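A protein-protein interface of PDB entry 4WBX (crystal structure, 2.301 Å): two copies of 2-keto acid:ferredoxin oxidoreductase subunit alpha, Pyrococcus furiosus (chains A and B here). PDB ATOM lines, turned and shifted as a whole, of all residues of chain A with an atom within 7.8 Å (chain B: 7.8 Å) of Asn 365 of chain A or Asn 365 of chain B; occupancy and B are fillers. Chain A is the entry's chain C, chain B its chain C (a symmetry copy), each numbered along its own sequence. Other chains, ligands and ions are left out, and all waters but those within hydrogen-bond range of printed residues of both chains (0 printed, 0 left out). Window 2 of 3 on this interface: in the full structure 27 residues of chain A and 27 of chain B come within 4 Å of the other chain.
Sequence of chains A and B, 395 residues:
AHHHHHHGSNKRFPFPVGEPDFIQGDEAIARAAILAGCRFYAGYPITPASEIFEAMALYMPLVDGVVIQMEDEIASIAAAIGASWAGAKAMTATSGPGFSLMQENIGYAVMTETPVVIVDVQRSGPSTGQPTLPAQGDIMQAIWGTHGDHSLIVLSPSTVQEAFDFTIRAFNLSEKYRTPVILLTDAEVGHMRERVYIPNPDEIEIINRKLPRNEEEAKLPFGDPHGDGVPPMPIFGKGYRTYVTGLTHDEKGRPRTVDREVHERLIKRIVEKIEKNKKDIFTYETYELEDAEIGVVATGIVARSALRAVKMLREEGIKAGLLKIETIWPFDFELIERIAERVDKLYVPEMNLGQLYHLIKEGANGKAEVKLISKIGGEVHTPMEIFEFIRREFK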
ATOM      1  N   PHE A 333     -27.951  -3.626  -0.099  1.00  0.00           N
ATOM      2  CA  PHE A 333     -27.752  -4.244   1.204  1.00  0.00           C
ATOM      3  C   PHE A 333     -27.859  -3.201   2.328  1.00  0.00           C
ATOM      4  O   PHE A 333     -28.517  -3.442   3.350  1.00  0.00           O
ATOM      5  CB  PHE A 333     -26.398  -4.977   1.243  1.00  0.00           C
ATOM      6  CG  PHE A 333     -26.410  -6.328   0.543  1.00  0.00           C
ATOM      7  CD1 PHE A 333     -26.851  -7.472   1.209  1.00  0.00           C
ATOM      8  CD2 PHE A 333     -25.976  -6.455  -0.776  1.00  0.00           C
ATOM      9  CE1 PHE A 333     -26.861  -8.720   0.576  1.00  0.00           C
ATOM     10  CE2 PHE A 333     -25.988  -7.701  -1.418  1.00  0.00           C
ATOM     11  CZ  PHE A 333     -26.431  -8.831  -0.736  1.00  0.00           C
ATOM     12  N   ILE A 336     -31.383  -2.312   3.662  1.00  0.00           N
ATOM     13  CA  ILE A 336     -31.917  -3.279   4.621  1.00  0.00           C
ATOM     14  C   ILE A 336     -31.256  -3.055   5.984  1.00  0.00           C
ATOM     15  O   ILE A 336     -31.855  -3.315   7.026  1.00  0.00           O
ATOM     16  CB  ILE A 336     -31.686  -4.741   4.161  1.00  0.00           C
ATOM     17  CG1 ILE A 336     -32.272  -4.966   2.769  1.00  0.00           C
ATOM     18  CG2 ILE A 336     -32.294  -5.731   5.139  1.00  0.00           C
ATOM     19  CD1 ILE A 336     -33.758  -4.813   2.696  1.00  0.00           C
ATOM     20  N   GLU A 337     -30.020  -2.566   5.958  1.00  0.00           N
ATOM     21  CA  GLU A 337     -29.286  -2.221   7.163  1.00  0.00           C
ATOM     22  C   GLU A 337     -29.999  -1.097   7.912  1.00  0.00           C
ATOM     23  O   GLU A 337     -30.408  -1.240   9.067  1.00  0.00           O
ATOM     24  CB  GLU A 337     -27.860  -1.816   6.784  1.00  0.00           C
ATOM     25  CG  GLU A 337     -27.034  -1.255   7.902  1.00  0.00           C
ATOM     26  CD  GLU A 337     -26.316  -2.345   8.646  1.00  0.00           C
ATOM     27  OE1 GLU A 337     -27.009  -3.176   9.274  1.00  0.00           O
ATOM     28  OE2 GLU A 337     -25.068  -2.379   8.594  1.00  0.00           O
ATOM     29  N   ARG A 338     -30.160   0.022   7.223  1.00  0.00           N
ATOM     30  CA  ARG A 338     -30.852   1.176   7.772  1.00  0.00           C
ATOM     31  C   ARG A 338     -32.224   0.823   8.334  1.00  0.00           C
ATOM     32  O   ARG A 338     -32.613   1.345   9.380  1.00  0.00           O
ATOM     33  CB  ARG A 338     -30.967   2.260   6.706  1.00  0.00           C
ATOM     34  CG  ARG A 338     -29.671   2.411   5.932  1.00  0.00           C
ATOM     35  CD  ARG A 338     -29.818   3.293   4.710  1.00  0.00           C
ATOM     36  NE  ARG A 338     -28.743   4.278   4.678  1.00  0.00           N
ATOM     37  CZ  ARG A 338     -28.676   5.290   3.822  1.00  0.00           C
ATOM     38  NH1 ARG A 338     -29.626   5.442   2.909  1.00  0.00           N
ATOM     39  NH2 ARG A 338     -27.660   6.145   3.886  1.00  0.00           N
ATOM     40  N   ALA A 340     -33.074  -2.224   9.388  1.00  0.00           N
ATOM     41  CA  ALA A 340     -32.827  -3.119  10.521  1.00  0.00           C
ATOM     42  C   ALA A 340     -32.807  -2.335  11.830  1.00  0.00           C
ATOM     43  O   ALA A 340     -33.566  -2.634  12.763  1.00  0.00           O
ATOM     44  CB  ALA A 340     -31.512  -3.879  10.339  1.00  0.00           C
ATOM     45  N   GLU A 341     -31.930  -1.331  11.880  1.00  0.00           N
ATOM     46  CA  GLU A 341     -31.820  -0.436  13.029  1.00  0.00           C
ATOM     47  C   GLU A 341     -33.163   0.161  13.487  1.00  0.00           C
ATOM     48  O   GLU A 341     -33.476   0.140  14.676  1.00  0.00           O
ATOM     49  CB  GLU A 341     -30.842   0.685  12.703  1.00  0.00           C
ATOM     50  CG  GLU A 341     -29.423   0.210  12.570  1.00  0.00           C
ATOM     51  CD  GLU A 341     -28.647   1.065  11.623  1.00  0.00           C
ATOM     52  OE1 GLU A 341     -29.259   1.996  11.065  1.00  0.00           O
ATOM     53  OE2 GLU A 341     -27.442   0.805  11.425  1.00  0.00           O
ATOM     54  N   ILE A 360     -31.733 -10.740   3.194  1.00  0.00           N
ATOM     55  CA  ILE A 360     -32.212  -9.849   4.238  1.00  0.00           C
ATOM     56  C   ILE A 360     -31.289  -9.954   5.451  1.00  0.00           C
ATOM     57  O   ILE A 360     -30.716  -8.949   5.882  1.00  0.00           O
ATOM     58  CB  ILE A 360     -33.662 -10.155   4.637  1.00  0.00           C
ATOM     59  CG1 ILE A 360     -34.604 -10.003   3.435  1.00  0.00           C
ATOM     60  CG2 ILE A 360     -34.089  -9.228   5.759  1.00  0.00           C
ATOM     61  CD1 ILE A 360     -34.498  -8.679   2.712  1.00  0.00           C
ATOM     62  N   LYS A 361     -31.106 -11.170   5.968  1.00  0.00           N
ATOM     63  CA  LYS A 361     -30.198 -11.390   7.102  1.00  0.00           C
ATOM     64  C   LYS A 361     -28.755 -10.905   6.840  1.00  0.00           C
ATOM     65  O   LYS A 361     -28.077 -10.425   7.753  1.00  0.00           O
ATOM     66  CB  LYS A 361     -30.180 -12.869   7.504  1.00  0.00           C
ATOM     67  CG  LYS A 361     -29.318 -13.139   8.735  1.00  0.00           C
ATOM     68  CD  LYS A 361     -30.008 -14.030   9.755  1.00  0.00           C
ATOM     69  CE  LYS A 361     -29.395 -13.854  11.146  1.00  0.00           C
ATOM     70  NZ  LYS A 361     -29.941 -14.852  12.113  1.00  0.00           N
ATOM     71  N   GLU A 362     -28.282 -11.012   5.607  1.00  0.00           N
ATOM     72  CA  GLU A 362     -26.964 -10.490   5.287  1.00  0.00           C
ATOM     73  C   GLU A 362     -27.046  -8.969   5.199  1.00  0.00           C
ATOM     74  O   GLU A 362     -26.055  -8.260   5.406  1.00  0.00           O
ATOM     75  CB  GLU A 362     -26.436 -11.089   3.983  1.00  0.00           C
ATOM     76  CG  GLU A 362     -25.174 -10.422   3.431  1.00  0.00           C
ATOM     77  CD  GLU A 362     -24.754 -10.993   2.090  1.00  0.00           C
ATOM     78  OE1 GLU A 362     -25.277 -12.070   1.717  1.00  0.00           O
ATOM     79  OE2 GLU A 362     -23.909 -10.371   1.403  1.00  0.00           O
ATOM     80  N   GLY A 363     -28.237  -8.463   4.901  1.00  0.00           N
ATOM     81  CA  GLY A 363     -28.426  -7.029   4.795  1.00  0.00           C
ATOM     82  C   GLY A 363     -28.464  -6.435   6.187  1.00  0.00           C
ATOM     83  O   GLY A 363     -27.802  -5.437   6.471  1.00  0.00           O
ATOM     84  N   ALA A 364     -29.247  -7.069   7.057  1.00  0.00           N
ATOM     85  CA  ALA A 364     -29.350  -6.667   8.451  1.00  0.00           C
ATOM     86  C   ALA A 364     -28.097  -7.099   9.187  1.00  0.00           C
ATOM     87  O   ALA A 364     -27.997  -8.247   9.628  1.00  0.00           O
ATOM     88  CB  ALA A 364     -30.597  -7.281   9.098  1.00  0.00           C
ATOM     89  N   ASN A 365     -27.144  -6.179   9.330  1.00  0.00           N
ATOM     90  CA  ASN A 365     -25.838  -6.491   9.919  1.00  0.00           C
ATOM     91  C   ASN A 365     -25.930  -6.883  11.381  1.00  0.00           C
ATOM     92  O   ASN A 365     -25.172  -6.374  12.199  1.00  0.00           O
ATOM     93  CB  ASN A 365     -24.896  -5.295   9.789  1.00  0.00           C
ATOM     94  CG  ASN A 365     -23.481  -5.698   9.478  1.00  0.00           C
ATOM     95  OD1 ASN A 365     -23.111  -6.857   9.632  1.00  0.00           O
ATOM     96  ND2 ASN A 365     -22.676  -4.740   9.024  1.00  0.00           N
ATOM     97  N   GLY A 366     -26.865  -7.774  11.702  1.00  0.00           N
ATOM     98  CA  GLY A 366     -27.149  -8.150  13.075  1.00  0.00           C
ATOM     99  C   GLY A 366     -28.113  -7.224  13.786  1.00  0.00           C
ATOM    100  O   GLY A 366     -28.600  -7.541  14.875  1.00  0.00           O
ATOM    101  N   LYS A 367     -28.408  -6.091  13.153  1.00  0.00           N
ATOM    102  CA  LYS A 367     -29.125  -5.000  13.805  1.00  0.00           C
ATOM    103  C   LYS A 367     -30.648  -5.162  13.829  1.00  0.00           C
ATOM    104  O   LYS A 367     -31.370  -4.172  13.986  1.00  0.00           O
ATOM    105  CB  LYS A 367     -28.758  -3.680  13.127  1.00  0.00           C
ATOM    106  CG  LYS A 367     -27.258  -3.454  13.062  1.00  0.00           C
ATOM    107  CD  LYS A 367     -26.918  -2.151  12.382  1.00  0.00           C
ATOM    108  CE  LYS A 367     -25.409  -1.938  12.319  1.00  0.00           C
ATOM    109  NZ  LYS A 367     -24.985  -0.628  12.905  1.00  0.00           N
ATOM    110  N   ALA A 368     -31.123  -6.400  13.679  1.00  0.00           N
ATOM    111  CA  ALA A 368     -32.541  -6.744  13.845  1.00  0.00           C
ATOM    112  C   ALA A 368     -32.707  -8.245  13.696  1.00  0.00           C
ATOM    113  O   ALA A 368     -31.959  -8.871  12.954  1.00  0.00           O
ATOM    114  CB  ALA A 368     -33.412  -6.017  12.835  1.00  0.00           C
ATOM    115  N   GLU A 369     -33.672  -8.830  14.397  1.00  0.00           N
ATOM    116  CA  GLU A 369     -33.946 -10.253  14.219  1.00  0.00           C
ATOM    117  C   GLU A 369     -34.640 -10.444  12.874  1.00  0.00           C
ATOM    118  O   GLU A 369     -35.489  -9.641  12.487  1.00  0.00           O
ATOM    119  CB  GLU A 369     -34.798 -10.816  15.362  1.00  0.00           C
ATOM    120  N   VAL A 370     -34.255 -11.492  12.151  1.00  0.00           N
ATOM    121  CA  VAL A 370     -34.793 -11.744  10.819  1.00  0.00           C
ATOM    122  C   VAL A 370     -35.431 -13.132  10.763  1.00  0.00           C
ATOM    123  O   VAL A 370     -34.777 -14.132  11.042  1.00  0.00           O
ATOM    124  CB  VAL A 370     -33.695 -11.614   9.751  1.00  0.00           C
ATOM    125  CG1 VAL A 370     -34.272 -11.854   8.376  1.00  0.00           C
ATOM    126  CG2 VAL A 370     -33.055 -10.240   9.819  1.00  0.00           C
ATOM    127  N   PHE B 333     -23.494 -21.504   9.673  1.00  0.00           N
ATOM    128  CA  PHE B 333     -23.532 -20.055   9.816  1.00  0.00           C
ATOM    129  C   PHE B 333     -23.141 -19.634  11.242  1.00  0.00           C
ATOM    130  O   PHE B 333     -22.348 -18.700  11.426  1.00  0.00           O
ATOM    131  CB  PHE B 333     -24.924 -19.520   9.432  1.00  0.00           C
ATOM    132  CG  PHE B 333     -25.159 -19.434   7.932  1.00  0.00           C
ATOM    133  CD1 PHE B 333     -24.723 -18.324   7.205  1.00  0.00           C
ATOM    134  CD2 PHE B 333     -25.815 -20.457   7.248  1.00  0.00           C
ATOM    135  CE1 PHE B 333     -24.939 -18.233   5.826  1.00  0.00           C
ATOM    136  CE2 PHE B 333     -26.030 -20.373   5.866  1.00  0.00           C
ATOM    137  CZ  PHE B 333     -25.589 -19.258   5.159  1.00  0.00           C
ATOM    138  N   ILE B 336     -19.376 -19.282  12.070  1.00  0.00           N
ATOM    139  CA  ILE B 336     -18.785 -18.020  11.623  1.00  0.00           C
ATOM    140  C   ILE B 336     -19.185 -16.904  12.592  1.00  0.00           C
ATOM    141  O   ILE B 336     -18.449 -15.937  12.780  1.00  0.00           O
ATOM    142  CB  ILE B 336     -19.227 -17.649  10.184  1.00  0.00           C
ATOM    143  CG1 ILE B 336     -18.905 -18.781   9.213  1.00  0.00           C
ATOM    144  CG2 ILE B 336     -18.562 -16.366   9.716  1.00  0.00           C
ATOM    145  CD1 ILE B 336     -17.443 -19.063   9.061  1.00  0.00           C
ATOM    146  N   GLU B 337     -20.356 -17.057  13.203  1.00  0.00           N
ATOM    147  CA  GLU B 337     -20.843 -16.131  14.211  1.00  0.00           C
ATOM    148  C   GLU B 337     -19.911 -16.130  15.421  1.00  0.00           C
ATOM    149  O   GLU B 337     -19.331 -15.107  15.797  1.00  0.00           O
ATOM    150  CB  GLU B 337     -22.266 -16.525  14.609  1.00  0.00           C
ATOM    151  CG  GLU B 337     -22.838 -15.774  15.774  1.00  0.00           C
ATOM    152  CD  GLU B 337     -23.523 -14.515  15.325  1.00  0.00           C
ATOM    153  OE1 GLU B 337     -22.818 -13.621  14.806  1.00  0.00           O
ATOM    154  OE2 GLU B 337     -24.760 -14.424  15.478  1.00  0.00           O
ATOM    155  N   ARG B 338     -19.761 -17.303  16.015  1.00  0.00           N
ATOM    156  CA  ARG B 338     -18.880 -17.486  17.156  1.00  0.00           C
ATOM    157  C   ARG B 338     -17.474 -16.957  16.902  1.00  0.00           C
ATOM    158  O   ARG B 338     -16.868 -16.364  17.796  1.00  0.00           O
ATOM    159  CB  ARG B 338     -18.841 -18.961  17.543  1.00  0.00           C
ATOM    160  CG  ARG B 338     -20.227 -19.577  17.508  1.00  0.00           C
ATOM    161  CD  ARG B 338     -20.202 -21.085  17.640  1.00  0.00           C
ATOM    162  NE  ARG B 338     -21.168 -21.510  18.646  1.00  0.00           N
ATOM    163  CZ  ARG B 338     -21.280 -22.750  19.104  1.00  0.00           C
ATOM    164  NH1 ARG B 338     -20.485 -23.700  18.629  1.00  0.00           N
ATOM    165  NH2 ARG B 338     -22.184 -23.034  20.036  1.00  0.00           N
ATOM    166  N   ALA B 340     -16.755 -14.588  14.669  1.00  0.00           N
ATOM    167  CA  ALA B 340     -16.895 -13.138  14.498  1.00  0.00           C
ATOM    168  C   ALA B 340     -16.622 -12.415  15.815  1.00  0.00           C
ATOM    169  O   ALA B 340     -15.751 -11.538  15.889  1.00  0.00           O
ATOM    170  CB  ALA B 340     -18.289 -12.783  13.978  1.00  0.00           C
ATOM    171  N   GLU B 341     -17.378 -12.799  16.844  1.00  0.00           N
ATOM    172  CA  GLU B 341     -17.210 -12.260  18.191  1.00  0.00           C
ATOM    173  C   GLU B 341     -15.759 -12.300  18.703  1.00  0.00           C
ATOM    174  O   GLU B 341     -15.256 -11.302  19.215  1.00  0.00           O
ATOM    175  CB  GLU B 341     -18.117 -13.016  19.153  1.00  0.00           C
ATOM    176  CG  GLU B 341     -19.577 -12.753  18.918  1.00  0.00           C
ATOM    177  CD  GLU B 341     -20.415 -13.924  19.314  1.00  0.00           C
ATOM    178  OE1 GLU B 341     -19.817 -14.934  19.736  1.00  0.00           O
ATOM    179  OE2 GLU B 341     -21.655 -13.846  19.195  1.00  0.00           O
ATOM    180  N   ILE B 360     -19.915 -15.430   4.569  1.00  0.00           N
ATOM    181  CA  ILE B 360     -19.186 -15.036   5.764  1.00  0.00           C
ATOM    182  C   ILE B 360     -19.900 -13.856   6.422  1.00  0.00           C
ATOM    183  O   ILE B 360     -20.294 -13.944   7.588  1.00  0.00           O
ATOM    184  CB  ILE B 360     -17.725 -14.677   5.456  1.00  0.00           C
ATOM    185  CG1 ILE B 360     -16.986 -15.873   4.841  1.00  0.00           C
ATOM    186  CG2 ILE B 360     -17.031 -14.229   6.728  1.00  0.00           C
ATOM    187  CD1 ILE B 360     -17.084 -17.154   5.637  1.00  0.00           C
ATOM    188  N   LYS B 361     -20.109 -12.777   5.665  1.00  0.00           N
ATOM    189  CA  LYS B 361     -20.834 -11.609   6.183  1.00  0.00           C
ATOM    190  C   LYS B 361     -22.246 -11.942   6.709  1.00  0.00           C
ATOM    191  O   LYS B 361     -22.714 -11.340   7.680  1.00  0.00           O
ATOM    192  CB  LYS B 361     -20.926 -10.511   5.117  1.00  0.00           C
ATOM    193  CG  LYS B 361     -21.593  -9.238   5.633  1.00  0.00           C
ATOM    194  CD  LYS B 361     -20.831  -7.978   5.255  1.00  0.00           C
ATOM    195  CE  LYS B 361     -21.184  -6.818   6.189  1.00  0.00           C
ATOM    196  NZ  LYS B 361     -20.583  -5.536   5.717  1.00  0.00           N
ATOM    197  N   GLU B 362     -22.926 -12.898   6.092  1.00  0.00           N
ATOM    198  CA  GLU B 362     -24.223 -13.310   6.601  1.00  0.00           C
ATOM    199  C   GLU B 362     -24.012 -14.167   7.846  1.00  0.00           C
ATOM    200  O   GLU B 362     -24.882 -14.255   8.719  1.00  0.00           O
ATOM    201  CB  GLU B 362     -25.016 -14.072   5.538  1.00  0.00           C
ATOM    202  CG  GLU B 362     -26.282 -14.763   6.048  1.00  0.00           C
ATOM    203  CD  GLU B 362     -26.971 -15.580   4.972  1.00  0.00           C
ATOM    204  OE1 GLU B 362     -26.623 -15.402   3.781  1.00  0.00           O
ATOM    205  OE2 GLU B 362     -27.856 -16.403   5.308  1.00  0.00           O
ATOM    206  N   GLY B 363     -22.844 -14.793   7.935  1.00  0.00           N
ATOM    207  CA  GLY B 363     -22.539 -15.632   9.079  1.00  0.00           C
ATOM    208  C   GLY B 363     -22.214 -14.745  10.263  1.00  0.00           C
ATOM    209  O   GLY B 363     -22.721 -14.946  11.366  1.00  0.00           O
ATOM    210  N   ALA B 364     -21.362 -13.753  10.017  1.00  0.00           N
ATOM    211  CA  ALA B 364     -20.990 -12.774  11.026  1.00  0.00           C
ATOM    212  C   ALA B 364     -22.139 -11.805  11.226  1.00  0.00           C
ATOM    213  O   ALA B 364     -22.273 -10.835  10.476  1.00  0.00           O
ATOM    214  CB  ALA B 364     -19.718 -12.028  10.611  1.00  0.00           C
ATOM    215  N   ASN B 365     -22.962 -12.060  12.241  1.00  0.00           N
ATOM    216  CA  ASN B 365     -24.177 -11.272  12.480  1.00  0.00           C
ATOM    217  C   ASN B 365     -23.881  -9.830  12.846  1.00  0.00           C
ATOM    218  O   ASN B 365     -24.440  -9.317  13.808  1.00  0.00           O
ATOM    219  CB  ASN B 365     -25.008 -11.902  13.596  1.00  0.00           C
ATOM    220  CG  ASN B 365     -26.487 -11.828  13.334  1.00  0.00           C
ATOM    221  OD1 ASN B 365     -26.936 -11.072  12.479  1.00  0.00           O
ATOM    222  ND2 ASN B 365     -27.261 -12.626  14.066  1.00  0.00           N
ATOM    223  N   GLY B 366     -22.995  -9.192  12.085  1.00  0.00           N
ATOM    224  CA  GLY B 366     -22.523  -7.853  12.389  1.00  0.00           C
ATOM    225  C   GLY B 366     -21.371  -7.808  13.369  1.00  0.00           C
ATOM    226  O   GLY B 366     -20.742  -6.761  13.550  1.00  0.00           O
ATOM    227  N   LYS B 367     -21.078  -8.953  13.979  1.00  0.00           N
ATOM    228  CA  LYS B 367     -20.162  -9.019  15.113  1.00  0.00           C
ATOM    229  C   LYS B 367     -18.678  -9.062  14.733  1.00  0.00           C
ATOM    230  O   LYS B 367     -17.849  -9.499  15.537  1.00  0.00           O
ATOM    231  CB  LYS B 367     -20.508 -10.234  15.971  1.00  0.00           C
ATOM    232  CG  LYS B 367     -21.970 -10.262  16.382  1.00  0.00           C
ATOM    233  CD  LYS B 367     -22.292 -11.474  17.221  1.00  0.00           C
ATOM    234  CE  LYS B 367     -23.763 -11.492  17.623  1.00  0.00           C
ATOM    235  NZ  LYS B 367     -23.957 -11.616  19.102  1.00  0.00           N
ATOM    236  N   ALA B 368     -18.355  -8.605  13.521  1.00  0.00           N
ATOM    237  CA  ALA B 368     -16.970  -8.424  13.072  1.00  0.00           C
ATOM    238  C   ALA B 368     -16.974  -7.804  11.687  1.00  0.00           C
ATOM    239  O   ALA B 368     -17.891  -8.049  10.912  1.00  0.00           O
ATOM    240  CB  ALA B 368     -16.213  -9.741  13.055  1.00  0.00           C
ATOM    241  N   GLU B 369     -15.966  -6.998  11.370  1.00  0.00           N
ATOM    242  CA  GLU B 369     -15.863  -6.454  10.019  1.00  0.00           C
ATOM    243  C   GLU B 369     -15.423  -7.574   9.082  1.00  0.00           C
ATOM    244  O   GLU B 369     -14.579  -8.395   9.438  1.00  0.00           O
ATOM    245  CB  GLU B 369     -14.891  -5.271   9.955  1.00  0.00           C
ATOM    246  N   VAL B 370     -16.022  -7.623   7.894  1.00  0.00           N
ATOM    247  CA  VAL B 370     -15.739  -8.686   6.936  1.00  0.00           C
ATOM    248  C   VAL B 370     -15.256  -8.090   5.616  1.00  0.00           C
ATOM    249  O   VAL B 370     -15.946  -7.280   5.005  1.00  0.00           O
ATOM    250  CB  VAL B 370     -16.982  -9.562   6.707  1.00  0.00           C
ATOM    251  CG1 VAL B 370     -16.667 -10.671   5.732  1.00  0.00           C
ATOM    252  CG2 VAL B 370     -17.468 -10.141   8.023  1.00  0.00           C
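Lys 361 of chain A touches Asn 365 of chain B.
CB of Glu 362 of chain B touches CB of Glu 362 of chain A, at 3.7 Å.
Asn 365 of chain A touches Lys 361 of chain B (ND2 to CE, 3.8 Å).
Asn 365 of chain A touches just these residues of chain B: Lys 361, Asn 365 and Gly 366.
No residue of chain B comes within 4 Å of Ala 364 of chain A.
Printed residues of chain B within 4 Å of Lys 361 of chain A: Asn 365.
Of the printed residues of chain A, Glu 362 of chain B touches Glu 362.
Ile 360 of chain A touches none of the printed residues of chain B.
The nearest residue of chain A that does not touch Asn 365 of chain B is Ala 364 of chain A (4.2 Å).
The nearest printed residue of chain B that does not touch Glu 362 of chain A is Lys 361 of chain B (4.4 Å).
Printed residues of chain A that touch a printed residue of chain B: Lys 361, Glu 362, Asn 365 and Gly 366.
Among the printed residues, 6 pairs touch across the chains.
Among the printed residues, no Asp or Glu carboxylate lies within 4 Å of a Lys or Arg side-chain nitrogen of the other chain.
OD1 of Asn 365 of chain A lies close to N of Gly 366 of chain B, at 3.4 Å.
The backbone NH (N) of Gly 366 of chain A lies close to the side-chain amide oxygen (OD1) of Asn 365 of chain B (3.4 Å).
The backbone carbonyl oxygen of Asn 365 of chain B lies close to the backbone carbonyl oxygen of Asn 365 of chain A.
The side-chain carboxylate (OE1) of Glu 337 of chain A is in hydrogen-bond range of the backbone NH (N) of Asn 365 of chain A, 3.0 Å away.
The backbone NH of Asn 365 of chain B is in hydrogen-bond range of the side-chain carboxylate of Glu 337 of chain B.
Lys 361 of chain A touches Asn 365 of chain B, and with the chains exchanged Asn 365 of chain A touches Lys 361 of chain B.
Glu 362 of chain A touches its own counterpart, Glu 362 of chain B.
Asn 365 of chain A touches its own counterpart, Asn 365 of chain B.
Asn 365 of chain A touches Gly 366 of chain B, and with the chains exchanged Gly 366 of chain A touches Asn 365 of chain B.
17 positions are printed for both chains.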
